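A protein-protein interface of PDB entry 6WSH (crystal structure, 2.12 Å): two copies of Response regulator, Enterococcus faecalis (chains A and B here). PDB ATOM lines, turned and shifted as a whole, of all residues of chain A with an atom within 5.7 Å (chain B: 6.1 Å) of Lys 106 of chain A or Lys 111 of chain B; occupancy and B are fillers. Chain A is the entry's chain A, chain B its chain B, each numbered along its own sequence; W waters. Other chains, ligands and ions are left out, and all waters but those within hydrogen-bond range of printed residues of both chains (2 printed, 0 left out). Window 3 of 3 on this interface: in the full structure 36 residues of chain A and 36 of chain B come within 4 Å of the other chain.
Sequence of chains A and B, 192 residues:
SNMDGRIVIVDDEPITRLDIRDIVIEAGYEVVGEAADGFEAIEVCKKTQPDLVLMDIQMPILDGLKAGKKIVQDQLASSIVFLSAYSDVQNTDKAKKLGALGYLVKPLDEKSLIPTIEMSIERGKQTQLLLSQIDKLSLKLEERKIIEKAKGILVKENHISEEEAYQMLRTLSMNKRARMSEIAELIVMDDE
O of Pro 107 of chain A is in hydrogen-bond range of NZ of Lys 111 of chain B (2.9 Å). O of Val 105 of chain A sits close to NZ of Lys 111 of chain B (3.2 Å).
OD1 of Asp 109 of chain B is in salt-bridge range of NZ of Lys 111 of chain B (2.7 Å). The side-chain hydroxyl (OG) of Ser 112 of chain B lies within hydrogen-bond range of the side-chain carboxylate (OD2) of Asp 109 of chain B (2.6 Å). The side-chain carboxylate (OD2) of Asp 56 of chain A lies close to the side-chain amino group (NZ) of Lys 106 of chain A. NZ of Lys 106 of chain A is in salt-bridge range of OD2 of Asp 11 of chain A, at 2.7 Å. The side-chain hydroxyl (OG1) of Thr 116 of chain B is in hydrogen-bond range of the backbone carbonyl oxygen (O) of Ser 112 of chain B. The backbone NH of Lys 106 of chain A is in hydrogen-bond range of the backbone carbonyl oxygen of Ser 84 of chain A (2.9 Å).
Pro 115 of chain B touches Ser 87 of chain A. OG of Ser 112 of chain B touches N of Val 105 of chain A, 3.5 Å away. Val 105 of chain A touches Pro 115 of chain B (CG2 to CG, 3.7 Å). Lys 111 of chain B touches Lys 106 of chain A (CE to O, 3.3 Å). OD2 of Asp 109 of chain B touches CB of Asp 109 of chain A, at 3.6 Å.
Printed residues of chain A within 4 Å of Ser 112 of chain B: Val 105 (3.5 Å). Printed residues of chain A within 4 Å of Pro 115 of chain B: Ser 87 and Val 105. The nearest printed residue of chain B that does not touch Lys 106 of chain A is Ser 112 of chain B (6.1 Å). The nearest printed residue of chain A that does not touch Pro 115 of chain B is Leu 104 of chain A (5.1 Å).
Printed residues of chain B that touch a printed residue of chain A: Asp 109, Lys 111, Ser 112 and Pro 115. Hydrophobic or aromatic side chains of chain A within 4 Å of the printed part of chain B: Val 105. Among the printed residues, 7 pairs touch across the chains. Among the printed residues, no Asp or Glu carboxylate lies within 4 Å of a Lys or Arg side-chain nitrogen of the other chain.
Asp 109 of chain B touches its own counterpart, Asp 109 of chain A. 1 position is printed for both chains.
Water W1 bridges the backbone NH of Asp 109 of chain B (2.8 Å) and the side-chain carboxylate of Asp 109 of chain A (2.9 Å). Water W2 lies within hydrogen-bond range of the side-chain hydroxyl (OG) of Ser 112 of chain B (2.9 Å), the backbone carbonyl oxygen (O) of Val 105 of chain A (2.9 Å), the backbone NH (N) of Asp 109 of chain A (3.1 Å) and the side-chain carboxylate (OD2) of Asp 109 of chain B (3.1 Å).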
ATOM      1  N   ASP A  11      26.026  18.083   5.921  1.00  0.00           N
ATOM      2  CA  ASP A  11      26.237  17.955   4.477  1.00  0.00           C
ATOM      3  C   ASP A  11      27.520  17.145   4.274  1.00  0.00           C
ATOM      4  O   ASP A  11      28.479  17.315   5.030  1.00  0.00           O
ATOM      5  CB  ASP A  11      26.334  19.344   3.814  1.00  0.00           C
ATOM      6  CG  ASP A  11      26.209  19.287   2.307  1.00  0.00           C
ATOM      7  OD1 ASP A  11      26.845  18.409   1.690  1.00  0.00           O
ATOM      8  OD2 ASP A  11      25.454  20.106   1.749  1.00  0.00           O
ATOM      9  N   ASP A  12      27.521  16.248   3.279  1.00  0.00           N
ATOM     10  CA  ASP A  12      28.713  15.439   3.018  1.00  0.00           C
ATOM     11  C   ASP A  12      29.846  16.243   2.384  1.00  0.00           C
ATOM     12  O   ASP A  12      31.020  15.865   2.534  1.00  0.00           O
ATOM     13  CB  ASP A  12      28.327  14.187   2.219  1.00  0.00           C
ATOM     14  CG  ASP A  12      27.626  14.494   0.898  1.00  0.00           C
ATOM     15  OD1 ASP A  12      28.083  13.950  -0.147  1.00  0.00           O
ATOM     16  OD2 ASP A  12      26.642  15.238   0.901  1.00  0.00           O
ATOM     17  N   GLU A  13      29.537  17.328   1.688  1.00  0.00           N
ATOM     18  CA  GLU A  13      30.538  18.224   1.101  1.00  0.00           C
ATOM     19  C   GLU A  13      31.191  19.223   2.068  1.00  0.00           C
ATOM     20  O   GLU A  13      30.533  20.163   2.525  1.00  0.00           O
ATOM     21  CB  GLU A  13      29.884  19.006  -0.045  1.00  0.00           C
ATOM     22  CG  GLU A  13      29.716  18.294  -1.373  1.00  0.00           C
ATOM     23  CD  GLU A  13      29.214  19.260  -2.446  1.00  0.00           C
ATOM     24  OE1 GLU A  13      28.135  18.966  -3.011  1.00  0.00           O
ATOM     25  OE2 GLU A  13      29.852  20.309  -2.697  1.00  0.00           O
ATOM     26  N   THR A  16      30.549  22.931   1.026  1.00  0.00           N
ATOM     27  CA  THR A  16      29.201  23.422   1.274  1.00  0.00           C
ATOM     28  C   THR A  16      28.937  23.635   2.762  1.00  0.00           C
ATOM     29  O   THR A  16      28.315  24.643   3.154  1.00  0.00           O
ATOM     30  CB  THR A  16      28.185  22.438   0.699  1.00  0.00           C
ATOM     31  OG1 THR A  16      28.463  22.234  -0.698  1.00  0.00           O
ATOM     32  CG2 THR A  16      26.765  22.971   0.879  1.00  0.00           C
ATOM     33  N   ASP A  56      21.377  18.191   4.263  1.00  0.00           N
ATOM     34  CA  ASP A  56      21.263  17.633   2.922  1.00  0.00           C
ATOM     35  C   ASP A  56      20.518  16.301   2.992  1.00  0.00           C
ATOM     36  O   ASP A  56      20.652  15.537   3.959  1.00  0.00           O
ATOM     37  CB  ASP A  56      22.645  17.422   2.317  1.00  0.00           C
ATOM     38  CG  ASP A  56      22.607  17.209   0.806  1.00  0.00           C
ATOM     39  OD1 ASP A  56      21.510  16.953   0.270  1.00  0.00           O
ATOM     40  OD2 ASP A  56      23.662  17.350   0.155  1.00  0.00           O
ATOM     41  N   LEU A  83      18.184  20.768   2.573  1.00  0.00           N
ATOM     42  CA  LEU A  83      18.959  21.476   1.547  1.00  0.00           C
ATOM     43  C   LEU A  83      19.457  20.517   0.464  1.00  0.00           C
ATOM     44  O   LEU A  83      20.565  19.989   0.583  1.00  0.00           O
ATOM     45  CB  LEU A  83      20.134  22.174   2.226  1.00  0.00           C
ATOM     46  CG  LEU A  83      19.913  23.174   3.357  1.00  0.00           C
ATOM     47  CD1 LEU A  83      21.257  23.706   3.864  1.00  0.00           C
ATOM     48  CD2 LEU A  83      19.044  24.319   2.890  1.00  0.00           C
ATOM     49  N   SER A  84      18.640  20.260  -0.557  1.00  0.00           N
ATOM     50  CA  SER A  84      18.939  19.263  -1.577  1.00  0.00           C
ATOM     51  C   SER A  84      18.950  19.846  -2.986  1.00  0.00           C
ATOM     52  O   SER A  84      18.220  20.799  -3.296  1.00  0.00           O
ATOM     53  CB  SER A  84      17.924  18.107  -1.503  1.00  0.00           C
ATOM     54  OG  SER A  84      18.096  17.168  -2.551  1.00  0.00           O
ATOM     55  N   ALA A  85      19.806  19.254  -3.834  1.00  0.00           N
ATOM     56  CA  ALA A  85      19.710  19.488  -5.269  1.00  0.00           C
ATOM     57  C   ALA A  85      18.439  18.903  -5.870  1.00  0.00           C
ATOM     58  O   ALA A  85      18.128  19.195  -7.018  1.00  0.00           O
ATOM     59  CB  ALA A  85      20.912  18.888  -6.002  1.00  0.00           C
ATOM     60  N   SER A  87      14.252  18.181  -5.767  1.00  0.00           N
ATOM     61  CA  SER A  87      13.022  18.825  -5.327  1.00  0.00           C
ATOM     62  C   SER A  87      11.776  18.064  -5.773  1.00  0.00           C
ATOM     63  O   SER A  87      10.676  18.635  -5.768  1.00  0.00           O
ATOM     64  CB  SER A  87      12.986  20.268  -5.859  1.00  0.00           C
ATOM     65  OG  SER A  87      12.944  20.310  -7.285  1.00  0.00           O
ATOM     66  N   LEU A 104      14.709  23.801   0.960  1.00  0.00           N
ATOM     67  CA  LEU A 104      15.338  24.747   0.051  1.00  0.00           C
ATOM     68  C   LEU A 104      16.248  23.957  -0.876  1.00  0.00           C
ATOM     69  O   LEU A 104      16.787  22.915  -0.496  1.00  0.00           O
ATOM     70  CB  LEU A 104      16.142  25.802   0.802  1.00  0.00           C
ATOM     71  CG  LEU A 104      15.415  26.712   1.786  1.00  0.00           C
ATOM     72  CD1 LEU A 104      16.415  27.664   2.429  1.00  0.00           C
ATOM     73  CD2 LEU A 104      14.316  27.502   1.097  1.00  0.00           C
ATOM     74  N   VAL A 105      16.419  24.452  -2.097  1.00  0.00           N
ATOM     75  CA  VAL A 105      16.923  23.654  -3.211  1.00  0.00           C
ATOM     76  C   VAL A 105      18.234  24.259  -3.709  1.00  0.00           C
ATOM     77  O   VAL A 105      18.314  25.468  -3.955  1.00  0.00           O
ATOM     78  CB  VAL A 105      15.877  23.578  -4.339  1.00  0.00           C
ATOM     79  CG1 VAL A 105      16.466  22.868  -5.531  1.00  0.00           C
ATOM     80  CG2 VAL A 105      14.599  22.911  -3.814  1.00  0.00           C
ATOM     81  N   LYS A 106      19.266  23.408  -3.792  1.00  0.00           N
ATOM     82  CA  LYS A 106      20.598  23.784  -4.230  1.00  0.00           C
ATOM     83  C   LYS A 106      20.627  24.095  -5.725  1.00  0.00           C
ATOM     84  O   LYS A 106      19.824  23.563  -6.499  1.00  0.00           O
ATOM     85  CB  LYS A 106      21.566  22.655  -3.926  1.00  0.00           C
ATOM     86  CG  LYS A 106      21.868  22.460  -2.446  1.00  0.00           C
ATOM     87  CD  LYS A 106      22.783  21.251  -2.256  1.00  0.00           C
ATOM     88  CE  LYS A 106      23.297  21.143  -0.824  1.00  0.00           C
ATOM     89  NZ  LYS A 106      24.205  19.974  -0.639  1.00  0.00           N
ATOM     90  N   PRO A 107      21.550  24.971  -6.168  1.00  0.00           N
ATOM     91  CA  PRO A 107      22.438  25.817  -5.343  1.00  0.00           C
ATOM     92  C   PRO A 107      21.647  26.878  -4.569  1.00  0.00           C
ATOM     93  O   PRO A 107      20.729  27.510  -5.103  1.00  0.00           O
ATOM     94  CB  PRO A 107      23.380  26.432  -6.384  1.00  0.00           C
ATOM     95  CG  PRO A 107      22.625  26.433  -7.651  1.00  0.00           C
ATOM     96  CD  PRO A 107      21.767  25.193  -7.617  1.00  0.00           C
ATOM     97  N   LEU A 108      22.019  27.052  -3.308  1.00  0.00           N
ATOM     98  CA  LEU A 108      21.214  27.795  -2.350  1.00  0.00           C
ATOM     99  C   LEU A 108      21.038  29.261  -2.744  1.00  0.00           C
ATOM    100  O   LEU A 108      22.008  29.949  -3.079  1.00  0.00           O
ATOM    101  CB  LEU A 108      21.859  27.692  -0.966  1.00  0.00           C
ATOM    102  CG  LEU A 108      21.147  28.362   0.207  1.00  0.00           C
ATOM    103  CD1 LEU A 108      19.741  27.818   0.365  1.00  0.00           C
ATOM    104  CD2 LEU A 108      21.970  28.154   1.456  1.00  0.00           C
ATOM    105  N   ASP A 109      19.783  29.726  -2.724  1.00  0.00           N
ATOM    106  CA  ASP A 109      19.447  31.147  -2.718  1.00  0.00           C
ATOM    107  C   ASP A 109      19.734  31.757  -1.344  1.00  0.00           C
ATOM    108  O   ASP A 109      18.870  31.742  -0.451  1.00  0.00           O
ATOM    109  CB  ASP A 109      17.982  31.319  -3.110  1.00  0.00           C
ATOM    110  CG  ASP A 109      17.574  32.756  -3.195  1.00  0.00           C
ATOM    111  OD1 ASP A 109      18.330  33.554  -3.792  1.00  0.00           O
ATOM    112  OD2 ASP A 109      16.487  33.079  -2.674  1.00  0.00           O
ATOM    113  N   ASP B 109      13.530  32.748  -6.022  1.00  0.00           N
ATOM    114  CA  ASP B 109      14.110  31.449  -6.375  1.00  0.00           C
ATOM    115  C   ASP B 109      13.012  30.407  -6.594  1.00  0.00           C
ATOM    116  O   ASP B 109      12.579  29.717  -5.660  1.00  0.00           O
ATOM    117  CB  ASP B 109      15.084  31.009  -5.288  1.00  0.00           C
ATOM    118  CG  ASP B 109      15.857  29.769  -5.667  1.00  0.00           C
ATOM    119  OD1 ASP B 109      16.351  29.685  -6.817  1.00  0.00           O
ATOM    120  OD2 ASP B 109      15.980  28.869  -4.804  1.00  0.00           O
ATOM    121  N   GLU B 110      12.547  30.320  -7.841  1.00  0.00           N
ATOM    122  CA  GLU B 110      11.349  29.549  -8.162  1.00  0.00           C
ATOM    123  C   GLU B 110      11.467  28.081  -7.754  1.00  0.00           C
ATOM    124  O   GLU B 110      10.476  27.461  -7.348  1.00  0.00           O
ATOM    125  CB  GLU B 110      11.094  29.671  -9.673  1.00  0.00           C
ATOM    126  CG  GLU B 110      10.809  31.097 -10.133  1.00  0.00           C
ATOM    127  CD  GLU B 110      10.610  31.207 -11.636  1.00  0.00           C
ATOM    128  OE1 GLU B 110      10.144  30.224 -12.257  1.00  0.00           O
ATOM    129  OE2 GLU B 110      10.934  32.277 -12.188  1.00  0.00           O
ATOM    130  N   LYS B 111      12.656  27.500  -7.889  1.00  0.00           N
ATOM    131  CA  LYS B 111      12.855  26.105  -7.508  1.00  0.00           C
ATOM    132  C   LYS B 111      12.573  25.849  -6.028  1.00  0.00           C
ATOM    133  O   LYS B 111      12.081  24.774  -5.655  1.00  0.00           O
ATOM    134  CB  LYS B 111      14.268  25.699  -7.917  1.00  0.00           C
ATOM    135  CG  LYS B 111      15.398  26.380  -7.146  1.00  0.00           C
ATOM    136  CD  LYS B 111      16.747  26.106  -7.828  1.00  0.00           C
ATOM    137  CE  LYS B 111      17.948  26.286  -6.902  1.00  0.00           C
ATOM    138  NZ  LYS B 111      18.062  27.658  -6.324  1.00  0.00           N
ATOM    139  N   SER B 112      12.909  26.800  -5.172  1.00  0.00           N
ATOM    140  CA  SER B 112      12.557  26.692  -3.768  1.00  0.00           C
ATOM    141  C   SER B 112      11.065  26.865  -3.491  1.00  0.00           C
ATOM    142  O   SER B 112      10.574  26.361  -2.473  1.00  0.00           O
ATOM    143  CB  SER B 112      13.369  27.712  -2.973  1.00  0.00           C
ATOM    144  OG  SER B 112      14.757  27.429  -3.054  1.00  0.00           O
ATOM    145  N   LEU B 113      10.336  27.616  -4.315  1.00  0.00           N
ATOM    146  CA  LEU B 113       8.940  27.904  -3.988  1.00  0.00           C
ATOM    147  C   LEU B 113       8.082  26.655  -3.789  1.00  0.00           C
ATOM    148  O   LEU B 113       7.345  26.555  -2.790  1.00  0.00           O
ATOM    149  CB  LEU B 113       8.345  28.798  -5.067  1.00  0.00           C
ATOM    150  CG  LEU B 113       6.874  29.137  -4.836  1.00  0.00           C
ATOM    151  CD1 LEU B 113       6.672  29.977  -3.577  1.00  0.00           C
ATOM    152  CD2 LEU B 113       6.263  29.831  -6.065  1.00  0.00           C
ATOM    153  N   ILE B 114       8.120  25.709  -4.725  1.00  0.00           N
ATOM    154  CA  ILE B 114       7.261  24.531  -4.605  1.00  0.00           C
ATOM    155  C   ILE B 114       7.579  23.710  -3.360  1.00  0.00           C
ATOM    156  O   ILE B 114       6.639  23.335  -2.631  1.00  0.00           O
ATOM    157  CB  ILE B 114       7.329  23.699  -5.896  1.00  0.00           C
ATOM    158  CG1 ILE B 114       6.979  24.553  -7.126  1.00  0.00           C
ATOM    159  CG2 ILE B 114       6.424  22.503  -5.828  1.00  0.00           C
ATOM    160  CD1 ILE B 114       5.570  25.160  -7.085  1.00  0.00           C
ATOM    161  N   PRO B 115       8.834  23.359  -3.078  1.00  0.00           N
ATOM    162  CA  PRO B 115       9.107  22.682  -1.795  1.00  0.00           C
ATOM    163  C   PRO B 115       8.663  23.462  -0.562  1.00  0.00           C
ATOM    164  O   PRO B 115       8.150  22.855   0.398  1.00  0.00           O
ATOM    165  CB  PRO B 115      10.630  22.483  -1.840  1.00  0.00           C
ATOM    166  CG  PRO B 115      10.970  22.410  -3.338  1.00  0.00           C
ATOM    167  CD  PRO B 115      10.036  23.442  -3.950  1.00  0.00           C
ATOM    168  N   THR B 116       8.857  24.784  -0.558  1.00  0.00           N
ATOM    169  CA  THR B 116       8.423  25.576   0.584  1.00  0.00           C
ATOM    170  C   THR B 116       6.909  25.530   0.764  1.00  0.00           C
ATOM    171  O   THR B 116       6.404  25.428   1.896  1.00  0.00           O
ATOM    172  CB  THR B 116       8.884  27.021   0.405  1.00  0.00           C
ATOM    173  OG1 THR B 116      10.322  27.064   0.331  1.00  0.00           O
ATOM    174  CG2 THR B 116       8.399  27.879   1.559  1.00  0.00           C
HETATM  175  O   HOH W   1      13.732  33.593  -3.350  1.00  0.00           O
HETATM  176  O   HOH W   2      17.500  27.712  -2.315  1.00  0.00           O
